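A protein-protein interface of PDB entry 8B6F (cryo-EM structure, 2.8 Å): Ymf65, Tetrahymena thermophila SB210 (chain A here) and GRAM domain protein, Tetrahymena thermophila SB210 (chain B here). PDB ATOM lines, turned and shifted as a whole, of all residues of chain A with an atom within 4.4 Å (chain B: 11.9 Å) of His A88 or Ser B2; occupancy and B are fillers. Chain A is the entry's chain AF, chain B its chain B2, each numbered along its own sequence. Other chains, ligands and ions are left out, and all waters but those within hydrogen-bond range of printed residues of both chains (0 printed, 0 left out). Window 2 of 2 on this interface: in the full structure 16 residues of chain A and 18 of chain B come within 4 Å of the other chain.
No residue of chain B comes within 4 Å of Phe A84. Of chain B, only Ser B2 (3.8 Å) comes within 4 Å of His A88. No residue of chain B comes within 4 Å of Phe A89. No residue of chain B comes within 4 Å of Thr A146. No residue of chain B comes within 4 Å of Thr A149. Gly A219 touches just these residues of chain B: Tyr B43 and His B47. Thr A221 touches one residue of chain B. Ser B2 touches just these residues of chain A: His A88 (3.8 Å), Phe A215 (3.7 Å), Ser A220 (3.6 Å) and Thr A221 (3.6 Å). Of the printed residues of chain A, Tyr B3 touches Ser A220 (3.4 Å). Printed residues of chain A within 4 Å of Tyr B43: Gly A219. The nearest residue of chain B that does not touch His A88 is Tyr B3 (6.6 Å).
CE1 of His A88 touches CB of Ser B2, 3.8 Å away. Ser B2 touches Phe A215 (N to CZ, 3.7 Å). His B47 touches Phe A215 (NE2 to O, 3.7 Å). Gly A219 touches His B47 (CA to CE1, 3.7 Å). C of Ser B2 touches CB of Ser A220, 3.6 Å away. Ser A220 touches Tyr B3. Thr A221 touches Ser B2 (CG2 to N, 3.6 Å).
Printed residues of chain A that touch a printed residue of chain B: His A88, Phe A215, Gly A219, Ser A220 and Thr A221. Hydrophobic or aromatic side chains of chain A that line the printed part of chain B: His A88 and Phe A215. Of the 15 printed residues of chain B, 4 touch a printed residue of chain A. Hydrophobic or aromatic side chains of chain B within 4 Å of the printed part of chain A: Tyr B3, Tyr B43 and His B47. Among the printed residues, 8 pairs touch across the chains. Among the printed residues, no Asp or Glu carboxylate lies within 4 Å of a Lys or Arg side-chain nitrogen of the other chain.
The backbone NH of Gly A219 is in hydrogen-bond range of the side-chain hydroxyl of Tyr B43, 3.1 Å away.
The backbone carbonyl oxygen (O) of Trp A86 lies within hydrogen-bond range of a ring nitrogen (ND1) of His A88 (2.8 Å). The backbone carbonyl oxygen (O) of His A88 sits at hydrogen-bond distance from the backbone NH (N) of Asn A145, 3.0 Å away. The side-chain hydroxyl (OH) of Tyr B3 lies within hydrogen-bond range of a ring nitrogen (ND1) of His B13 (3.0 Å). N of Leu B16 sits at hydrogen-bond distance from OH of Tyr B3.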
ATOM      1  N   PHE A  84      -8.177  -5.599   6.340  1.00  0.00           N
ATOM      2  CA  PHE A  84      -8.481  -6.104   5.011  1.00  0.00           C
ATOM      3  C   PHE A  84      -9.323  -7.368   5.116  1.00  0.00           C
ATOM      4  O   PHE A  84      -9.308  -8.073   6.126  1.00  0.00           O
ATOM      5  CB  PHE A  84      -7.202  -6.375   4.201  1.00  0.00           C
ATOM      6  CG  PHE A  84      -6.309  -7.429   4.792  1.00  0.00           C
ATOM      7  CD1 PHE A  84      -5.436  -7.119   5.820  1.00  0.00           C
ATOM      8  CD2 PHE A  84      -6.328  -8.724   4.302  1.00  0.00           C
ATOM      9  CE1 PHE A  84      -4.609  -8.086   6.358  1.00  0.00           C
ATOM     10  CE2 PHE A  84      -5.504  -9.693   4.835  1.00  0.00           C
ATOM     11  CZ  PHE A  84      -4.643  -9.375   5.864  1.00  0.00           C
ATOM     12  N   TRP A  85     -10.056  -7.644   4.038  1.00  0.00           N
ATOM     13  CA  TRP A  85     -10.947  -8.799   3.939  1.00  0.00           C
ATOM     14  C   TRP A  85     -12.029  -8.768   5.021  1.00  0.00           C
ATOM     15  O   TRP A  85     -12.097  -9.626   5.902  1.00  0.00           O
ATOM     16  CB  TRP A  85     -10.154 -10.107   3.995  1.00  0.00           C
ATOM     17  CG  TRP A  85     -10.950 -11.267   3.500  1.00  0.00           C
ATOM     18  CD1 TRP A  85     -11.446 -12.299   4.237  1.00  0.00           C
ATOM     19  CD2 TRP A  85     -11.364 -11.502   2.150  1.00  0.00           C
ATOM     20  NE1 TRP A  85     -12.137 -13.168   3.428  1.00  0.00           N
ATOM     21  CE2 TRP A  85     -12.100 -12.700   2.141  1.00  0.00           C
ATOM     22  CE3 TRP A  85     -11.177 -10.815   0.946  1.00  0.00           C
ATOM     23  CZ2 TRP A  85     -12.647 -13.229   0.975  1.00  0.00           C
ATOM     24  CZ3 TRP A  85     -11.722 -11.341  -0.211  1.00  0.00           C
ATOM     25  CH2 TRP A  85     -12.450 -12.536  -0.188  1.00  0.00           C
ATOM     26  N   TRP A  86     -12.884  -7.749   4.934  1.00  0.00           N
ATOM     27  CA  TRP A  86     -14.070  -7.633   5.779  1.00  0.00           C
ATOM     28  C   TRP A  86     -13.714  -7.348   7.232  1.00  0.00           C
ATOM     29  O   TRP A  86     -14.427  -7.764   8.146  1.00  0.00           O
ATOM     30  CB  TRP A  86     -14.939  -8.892   5.693  1.00  0.00           C
ATOM     31  CG  TRP A  86     -15.167  -9.355   4.293  1.00  0.00           C
ATOM     32  CD1 TRP A  86     -14.553 -10.397   3.665  1.00  0.00           C
ATOM     33  CD2 TRP A  86     -16.067  -8.784   3.337  1.00  0.00           C
ATOM     34  NE1 TRP A  86     -15.018 -10.514   2.379  1.00  0.00           N
ATOM     35  CE2 TRP A  86     -15.946  -9.534   2.152  1.00  0.00           C
ATOM     36  CE3 TRP A  86     -16.962  -7.711   3.369  1.00  0.00           C
ATOM     37  CZ2 TRP A  86     -16.689  -9.250   1.011  1.00  0.00           C
ATOM     38  CZ3 TRP A  86     -17.700  -7.429   2.234  1.00  0.00           C
ATOM     39  CH2 TRP A  86     -17.559  -8.197   1.070  1.00  0.00           C
ATOM     40  N   SER A  87     -12.614  -6.636   7.459  1.00  0.00           N
ATOM     41  CA  SER A  87     -12.173  -6.259   8.798  1.00  0.00           C
ATOM     42  C   SER A  87     -11.881  -7.469   9.672  1.00  0.00           C
ATOM     43  O   SER A  87     -11.943  -7.379  10.901  1.00  0.00           O
ATOM     44  CB  SER A  87     -13.205  -5.358   9.486  1.00  0.00           C
ATOM     45  OG  SER A  87     -13.423  -4.169   8.744  1.00  0.00           O
ATOM     46  N   HIS A  88     -11.561  -8.609   9.062  1.00  0.00           N
ATOM     47  CA  HIS A  88     -11.194  -9.796   9.819  1.00  0.00           C
ATOM     48  C   HIS A  88      -9.701  -9.892  10.080  1.00  0.00           C
ATOM     49  O   HIS A  88      -9.290 -10.648  10.964  1.00  0.00           O
ATOM     50  CB  HIS A  88     -11.663 -11.055   9.085  1.00  0.00           C
ATOM     51  CG  HIS A  88     -13.120 -11.346   9.265  1.00  0.00           C
ATOM     52  ND1 HIS A  88     -14.094 -10.381   9.130  1.00  0.00           N
ATOM     53  CD2 HIS A  88     -13.766 -12.491   9.579  1.00  0.00           C
ATOM     54  CE1 HIS A  88     -15.279 -10.921   9.349  1.00  0.00           C
ATOM     55  NE2 HIS A  88     -15.109 -12.201   9.623  1.00  0.00           N
ATOM     56  N   PHE A  89      -8.883  -9.144   9.343  1.00  0.00           N
ATOM     57  CA  PHE A  89      -7.442  -9.129   9.538  1.00  0.00           C
ATOM     58  C   PHE A  89      -6.964  -7.692   9.656  1.00  0.00           C
ATOM     59  O   PHE A  89      -7.427  -6.814   8.923  1.00  0.00           O
ATOM     60  CB  PHE A  89      -6.718  -9.828   8.386  1.00  0.00           C
ATOM     61  CG  PHE A  89      -6.997 -11.299   8.302  1.00  0.00           C
ATOM     62  CD1 PHE A  89      -8.072 -11.771   7.569  1.00  0.00           C
ATOM     63  CD2 PHE A  89      -6.185 -12.207   8.957  1.00  0.00           C
ATOM     64  CE1 PHE A  89      -8.329 -13.124   7.490  1.00  0.00           C
ATOM     65  CE2 PHE A  89      -6.437 -13.558   8.883  1.00  0.00           C
ATOM     66  CZ  PHE A  89      -7.511 -14.019   8.150  1.00  0.00           C
ATOM     67  N   LEU A 143      -2.043 -11.345  12.933  1.00  0.00           N
ATOM     68  CA  LEU A 143      -2.806 -10.535  11.995  1.00  0.00           C
ATOM     69  C   LEU A 143      -4.303 -10.599  12.256  1.00  0.00           C
ATOM     70  O   LEU A 143      -5.070  -9.935  11.552  1.00  0.00           O
ATOM     71  CB  LEU A 143      -2.510 -10.977  10.559  1.00  0.00           C
ATOM     72  CG  LEU A 143      -1.072 -10.745  10.087  1.00  0.00           C
ATOM     73  CD1 LEU A 143      -0.805 -11.509   8.806  1.00  0.00           C
ATOM     74  CD2 LEU A 143      -0.798  -9.264   9.887  1.00  0.00           C
ATOM     75  N   SER A 144      -4.734 -11.377  13.246  1.00  0.00           N
ATOM     76  CA  SER A 144      -6.151 -11.479  13.562  1.00  0.00           C
ATOM     77  C   SER A 144      -6.695 -10.133  14.014  1.00  0.00           C
ATOM     78  O   SER A 144      -6.082  -9.446  14.835  1.00  0.00           O
ATOM     79  CB  SER A 144      -6.364 -12.519  14.660  1.00  0.00           C
ATOM     80  OG  SER A 144      -5.813 -13.769  14.292  1.00  0.00           O
ATOM     81  N   ASN A 145      -7.857  -9.761  13.482  1.00  0.00           N
ATOM     82  CA  ASN A 145      -8.544  -8.544  13.886  1.00  0.00           C
ATOM     83  C   ASN A 145      -9.788  -8.808  14.718  1.00  0.00           C
ATOM     84  O   ASN A 145     -10.359  -7.860  15.263  1.00  0.00           O
ATOM     85  CB  ASN A 145      -8.940  -7.720  12.653  1.00  0.00           C
ATOM     86  CG  ASN A 145      -9.451  -6.344  13.014  1.00  0.00           C
ATOM     87  OD1 ASN A 145      -9.053  -5.766  14.023  1.00  0.00           O
ATOM     88  ND2 ASN A 145     -10.351  -5.815  12.196  1.00  0.00           N
ATOM     89  N   THR A 146     -10.223 -10.060  14.829  1.00  0.00           N
ATOM     90  CA  THR A 146     -11.393 -10.400  15.620  1.00  0.00           C
ATOM     91  C   THR A 146     -11.139 -11.703  16.365  1.00  0.00           C
ATOM     92  O   THR A 146     -10.324 -12.526  15.946  1.00  0.00           O
ATOM     93  CB  THR A 146     -12.647 -10.532  14.741  1.00  0.00           C
ATOM     94  OG1 THR A 146     -12.655 -11.804  14.084  1.00  0.00           O
ATOM     95  CG2 THR A 146     -12.700  -9.430  13.692  1.00  0.00           C
ATOM     96  N   THR A 149     -11.851 -14.875  14.099  1.00  0.00           N
ATOM     97  CA  THR A 149     -10.758 -15.334  13.247  1.00  0.00           C
ATOM     98  C   THR A 149      -9.595 -15.865  14.074  1.00  0.00           C
ATOM     99  O   THR A 149      -8.925 -16.819  13.667  1.00  0.00           O
ATOM    100  CB  THR A 149     -10.289 -14.208  12.324  1.00  0.00           C
ATOM    101  OG1 THR A 149      -9.226 -14.683  11.488  1.00  0.00           O
ATOM    102  CG2 THR A 149      -9.799 -13.022  13.119  1.00  0.00           C
ATOM    103  N   PHE A 215     -20.249 -11.619  21.452  1.00  0.00           N
ATOM    104  CA  PHE A 215     -21.176 -11.166  20.421  1.00  0.00           C
ATOM    105  C   PHE A 215     -22.466 -10.641  21.038  1.00  0.00           C
ATOM    106  O   PHE A 215     -23.016  -9.634  20.580  1.00  0.00           O
ATOM    107  CB  PHE A 215     -21.478 -12.305  19.446  1.00  0.00           C
ATOM    108  CG  PHE A 215     -20.640 -12.276  18.202  1.00  0.00           C
ATOM    109  CD1 PHE A 215     -20.893 -11.351  17.204  1.00  0.00           C
ATOM    110  CD2 PHE A 215     -19.606 -13.180  18.024  1.00  0.00           C
ATOM    111  CE1 PHE A 215     -20.126 -11.323  16.056  1.00  0.00           C
ATOM    112  CE2 PHE A 215     -18.836 -13.156  16.878  1.00  0.00           C
ATOM    113  CZ  PHE A 215     -19.096 -12.226  15.893  1.00  0.00           C
ATOM    114  N   GLY A 219     -22.268  -6.014  19.542  1.00  0.00           N
ATOM    115  CA  GLY A 219     -22.762  -6.531  18.280  1.00  0.00           C
ATOM    116  C   GLY A 219     -21.720  -7.234  17.434  1.00  0.00           C
ATOM    117  O   GLY A 219     -22.068  -8.034  16.562  1.00  0.00           O
ATOM    118  N   SER A 220     -20.446  -6.946  17.671  1.00  0.00           N
ATOM    119  CA  SER A 220     -19.344  -7.540  16.927  1.00  0.00           C
ATOM    120  C   SER A 220     -18.393  -8.236  17.891  1.00  0.00           C
ATOM    121  O   SER A 220     -18.601  -8.256  19.105  1.00  0.00           O
ATOM    122  CB  SER A 220     -18.597  -6.484  16.108  1.00  0.00           C
ATOM    123  OG  SER A 220     -17.995  -5.517  16.947  1.00  0.00           O
ATOM    124  N   THR A 221     -17.338  -8.820  17.324  1.00  0.00           N
ATOM    125  CA  THR A 221     -16.263  -9.418  18.103  1.00  0.00           C
ATOM    126  C   THR A 221     -14.902  -8.845  17.719  1.00  0.00           C
ATOM    127  O   THR A 221     -13.873  -9.434  18.070  1.00  0.00           O
ATOM    128  CB  THR A 221     -16.272 -10.945  17.948  1.00  0.00           C
ATOM    129  OG1 THR A 221     -15.389 -11.537  18.908  1.00  0.00           O
ATOM    130  CG2 THR A 221     -15.844 -11.357  16.559  1.00  0.00           C
ATOM    131  N   SER B   2     -17.260  -9.974  13.594  1.00  0.00           N
ATOM    132  CA  SER B   2     -17.424  -8.567  13.132  1.00  0.00           C
ATOM    133  C   SER B   2     -18.899  -8.210  12.995  1.00  0.00           C
ATOM    134  O   SER B   2     -19.764  -9.079  13.070  1.00  0.00           O
ATOM    135  CB  SER B   2     -16.709  -8.362  11.797  1.00  0.00           C
ATOM    136  OG  SER B   2     -16.869  -7.035  11.329  1.00  0.00           O
ATOM    137  N   TYR B   3     -19.185  -6.925  12.798  1.00  0.00           N
ATOM    138  CA  TYR B   3     -20.555  -6.456  12.607  1.00  0.00           C
ATOM    139  C   TYR B   3     -20.854  -6.490  11.113  1.00  0.00           C
ATOM    140  O   TYR B   3     -20.539  -5.549  10.381  1.00  0.00           O
ATOM    141  CB  TYR B   3     -20.736  -5.056  13.180  1.00  0.00           C
ATOM    142  CG  TYR B   3     -22.134  -4.517  13.013  1.00  0.00           C
ATOM    143  CD1 TYR B   3     -23.128  -4.828  13.930  1.00  0.00           C
ATOM    144  CD2 TYR B   3     -22.462  -3.702  11.939  1.00  0.00           C
ATOM    145  CE1 TYR B   3     -24.408  -4.343  13.786  1.00  0.00           C
ATOM    146  CE2 TYR B   3     -23.744  -3.212  11.785  1.00  0.00           C
ATOM    147  CZ  TYR B   3     -24.711  -3.541  12.711  1.00  0.00           C
ATOM    148  OH  TYR B   3     -25.986  -3.059  12.571  1.00  0.00           O
ATOM    149  N   SER B   4     -21.462  -7.584  10.656  1.00  0.00           N
ATOM    150  CA  SER B   4     -21.751  -7.735   9.234  1.00  0.00           C
ATOM    151  C   SER B   4     -22.747  -6.688   8.752  1.00  0.00           C
ATOM    152  O   SER B   4     -22.618  -6.163   7.641  1.00  0.00           O
ATOM    153  CB  SER B   4     -22.282  -9.136   8.960  1.00  0.00           C
ATOM    154  OG  SER B   4     -23.485  -9.340   9.668  1.00  0.00           O
ATOM    155  N   GLY B   5     -23.748  -6.375   9.568  1.00  0.00           N
ATOM    156  CA  GLY B   5     -24.769  -5.425   9.186  1.00  0.00           C
ATOM    157  C   GLY B   5     -25.918  -5.997   8.388  1.00  0.00           C
ATOM    158  O   GLY B   5     -26.700  -5.223   7.824  1.00  0.00           O
ATOM    159  N   TYR B   6     -26.047  -7.317   8.316  1.00  0.00           N
ATOM    160  CA  TYR B   6     -27.143  -7.966   7.615  1.00  0.00           C
ATOM    161  C   TYR B   6     -28.212  -8.430   8.600  1.00  0.00           C
ATOM    162  O   TYR B   6     -27.958  -8.610   9.792  1.00  0.00           O
ATOM    163  CB  TYR B   6     -26.640  -9.164   6.809  1.00  0.00           C
ATOM    164  CG  TYR B   6     -25.741  -8.805   5.654  1.00  0.00           C
ATOM    165  CD1 TYR B   6     -26.269  -8.355   4.452  1.00  0.00           C
ATOM    166  CD2 TYR B   6     -24.364  -8.933   5.757  1.00  0.00           C
ATOM    167  CE1 TYR B   6     -25.450  -8.032   3.390  1.00  0.00           C
ATOM    168  CE2 TYR B   6     -23.537  -8.614   4.702  1.00  0.00           C
ATOM    169  CZ  TYR B   6     -24.085  -8.164   3.521  1.00  0.00           C
ATOM    170  OH  TYR B   6     -23.263  -7.845   2.468  1.00  0.00           O
ATOM    171  N   SER B   7     -29.420  -8.623   8.078  1.00  0.00           N
ATOM    172  CA  SER B   7     -30.519  -9.164   8.860  1.00  0.00           C
ATOM    173  C   SER B   7     -30.558 -10.681   8.679  1.00  0.00           C
ATOM    174  O   SER B   7     -29.658 -11.278   8.084  1.00  0.00           O
ATOM    175  CB  SER B   7     -31.835  -8.503   8.459  1.00  0.00           C
ATOM    176  OG  SER B   7     -32.164  -8.791   7.112  1.00  0.00           O
ATOM    177  N   LEU B   8     -31.603 -11.323   9.195  1.00  0.00           N
ATOM    178  CA  LEU B   8     -31.734 -12.769   9.082  1.00  0.00           C
ATOM    179  C   LEU B   8     -32.361 -13.212   7.768  1.00  0.00           C
ATOM    180  O   LEU B   8     -32.486 -14.419   7.538  1.00  0.00           O
ATOM    181  CB  LEU B   8     -32.559 -13.315  10.251  1.00  0.00           C
ATOM    182  CG  LEU B   8     -31.999 -13.061  11.656  1.00  0.00           C
ATOM    183  CD1 LEU B   8     -32.789 -13.830  12.702  1.00  0.00           C
ATOM    184  CD2 LEU B   8     -30.520 -13.378  11.745  1.00  0.00           C
ATOM    185  N   HIS B  13     -29.277  -5.015   9.002  1.00  0.00           N
ATOM    186  CA  HIS B  13     -29.430  -5.157  10.438  1.00  0.00           C
ATOM    187  C   HIS B  13     -30.107  -3.911  11.004  1.00  0.00           C
ATOM    188  O   HIS B  13     -29.758  -2.789  10.622  1.00  0.00           O
ATOM    189  CB  HIS B  13     -28.062  -5.363  11.090  1.00  0.00           C
ATOM    190  CG  HIS B  13     -28.130  -5.888  12.488  1.00  0.00           C
ATOM    191  ND1 HIS B  13     -27.964  -5.082  13.593  1.00  0.00           N
ATOM    192  CD2 HIS B  13     -28.342  -7.137  12.963  1.00  0.00           C
ATOM    193  CE1 HIS B  13     -28.075  -5.811  14.688  1.00  0.00           C
ATOM    194  NE2 HIS B  13     -28.302  -7.062  14.334  1.00  0.00           N
ATOM    195  N   CYS B  15     -29.735  -2.343  13.685  1.00  0.00           N
ATOM    196  CA  CYS B  15     -28.820  -1.471  14.410  1.00  0.00           C
ATOM    197  C   CYS B  15     -27.858  -0.724  13.497  1.00  0.00           C
ATOM    198  O   CYS B  15     -27.050   0.067  13.994  1.00  0.00           O
ATOM    199  CB  CYS B  15     -28.013  -2.279  15.433  1.00  0.00           C
ATOM    200  SG  CYS B  15     -29.012  -3.126  16.668  1.00  0.00           S
ATOM    201  N   LEU B  16     -27.915  -0.954  12.185  1.00  0.00           N
ATOM    202  CA  LEU B  16     -26.908  -0.378  11.299  1.00  0.00           C
ATOM    203  C   LEU B  16     -26.855   1.140  11.368  1.00  0.00           C
ATOM    204  O   LEU B  16     -25.738   1.684  11.418  1.00  0.00           O
ATOM    205  CB  LEU B  16     -27.155  -0.845   9.859  1.00  0.00           C
ATOM    206  CG  LEU B  16     -26.155  -0.334   8.815  1.00  0.00           C
ATOM    207  CD1 LEU B  16     -24.749  -0.819   9.129  1.00  0.00           C
ATOM    208  CD2 LEU B  16     -26.562  -0.763   7.419  1.00  0.00           C
ATOM    209  N   TYR B  19     -25.064   2.020  14.588  1.00  0.00           N
ATOM    210  CA  TYR B  19     -23.671   1.593  14.514  1.00  0.00           C
ATOM    211  C   TYR B  19     -22.855   2.534  13.637  1.00  0.00           C
ATOM    212  O   TYR B  19     -21.731   2.906  13.990  1.00  0.00           O
ATOM    213  CB  TYR B  19     -23.597   0.162  13.986  1.00  0.00           C
ATOM    214  CG  TYR B  19     -22.198  -0.398  13.899  1.00  0.00           C
ATOM    215  CD1 TYR B  19     -21.613  -1.028  14.988  1.00  0.00           C
ATOM    216  CD2 TYR B  19     -21.468  -0.310  12.723  1.00  0.00           C
ATOM    217  CE1 TYR B  19     -20.337  -1.548  14.910  1.00  0.00           C
ATOM    218  CE2 TYR B  19     -20.193  -0.826  12.634  1.00  0.00           C
ATOM    219  CZ  TYR B  19     -19.633  -1.445  13.730  1.00  0.00           C
ATOM    220  OH  TYR B  19     -18.361  -1.961  13.644  1.00  0.00           O
ATOM    221  N   MET B  22     -22.290   5.774  15.548  1.00  0.00           N
ATOM    222  CA  MET B  22     -21.293   5.603  16.600  1.00  0.00           C
ATOM    223  C   MET B  22     -19.887   5.554  16.021  1.00  0.00           C
ATOM    224  O   MET B  22     -18.966   6.189  16.548  1.00  0.00           O
ATOM    225  CB  MET B  22     -21.589   4.326  17.384  1.00  0.00           C
ATOM    226  CG  MET B  22     -20.609   4.039  18.508  1.00  0.00           C
ATOM    227  SD  MET B  22     -20.923   2.461  19.319  1.00  0.00           S
ATOM    228  CE  MET B  22     -20.602   1.312  17.982  1.00  0.00           C
ATOM    229  N   LEU B  23     -19.700   4.804  14.934  1.00  0.00           N
ATOM    230  CA  LEU B  23     -18.378   4.708  14.327  1.00  0.00           C
ATOM    231  C   LEU B  23     -17.934   6.054  13.770  1.00  0.00           C
ATOM    232  O   LEU B  23     -16.765   6.433  13.905  1.00  0.00           O
ATOM    233  CB  LEU B  23     -18.382   3.642  13.235  1.00  0.00           C
ATOM    234  CG  LEU B  23     -17.011   3.184  12.734  1.00  0.00           C
ATOM    235  CD1 LEU B  23     -16.191   2.565  13.854  1.00  0.00           C
ATOM    236  CD2 LEU B  23     -17.169   2.203  11.591  1.00  0.00           C
ATOM    237  N   TYR B  43     -26.751   3.035  20.270  1.00  0.00           N
ATOM    238  CA  TYR B  43     -26.431   1.744  19.670  1.00  0.00           C
ATOM    239  C   TYR B  43     -26.629   0.616  20.672  1.00  0.00           C
ATOM    240  O   TYR B  43     -27.219  -0.421  20.350  1.00  0.00           O
ATOM    241  CB  TYR B  43     -24.995   1.751  19.146  1.00  0.00           C
ATOM    242  CG  TYR B  43     -24.465   0.371  18.830  1.00  0.00           C
ATOM    243  CD1 TYR B  43     -24.854  -0.299  17.679  1.00  0.00           C
ATOM    244  CD2 TYR B  43     -23.575  -0.261  19.688  1.00  0.00           C
ATOM    245  CE1 TYR B  43     -24.374  -1.558  17.393  1.00  0.00           C
ATOM    246  CE2 TYR B  43     -23.090  -1.519  19.410  1.00  0.00           C
ATOM    247  CZ  TYR B  43     -23.491  -2.162  18.261  1.00  0.00           C
ATOM    248  OH  TYR B  43     -23.007  -3.417  17.982  1.00  0.00           O
ATOM    249  N   HIS B  47     -29.310  -2.495  20.577  1.00  0.00           N
ATOM    250  CA  HIS B  47     -28.774  -3.849  20.604  1.00  0.00           C
ATOM    251  C   HIS B  47     -29.342  -4.680  21.749  1.00  0.00           C
ATOM    252  O   HIS B  47     -29.750  -5.825  21.543  1.00  0.00           O
ATOM    253  CB  HIS B  47     -27.246  -3.799  20.699  1.00  0.00           C
ATOM    254  CG  HIS B  47     -26.599  -5.147  20.711  1.00  0.00           C
ATOM    255  ND1 HIS B  47     -26.698  -6.029  19.656  1.00  0.00           N
ATOM    256  CD2 HIS B  47     -25.847  -5.767  21.649  1.00  0.00           C
ATOM    257  CE1 HIS B  47     -26.033  -7.133  19.945  1.00  0.00           C
ATOM    258  NE2 HIS B  47     -25.507  -7.000  21.148  1.00  0.00           N
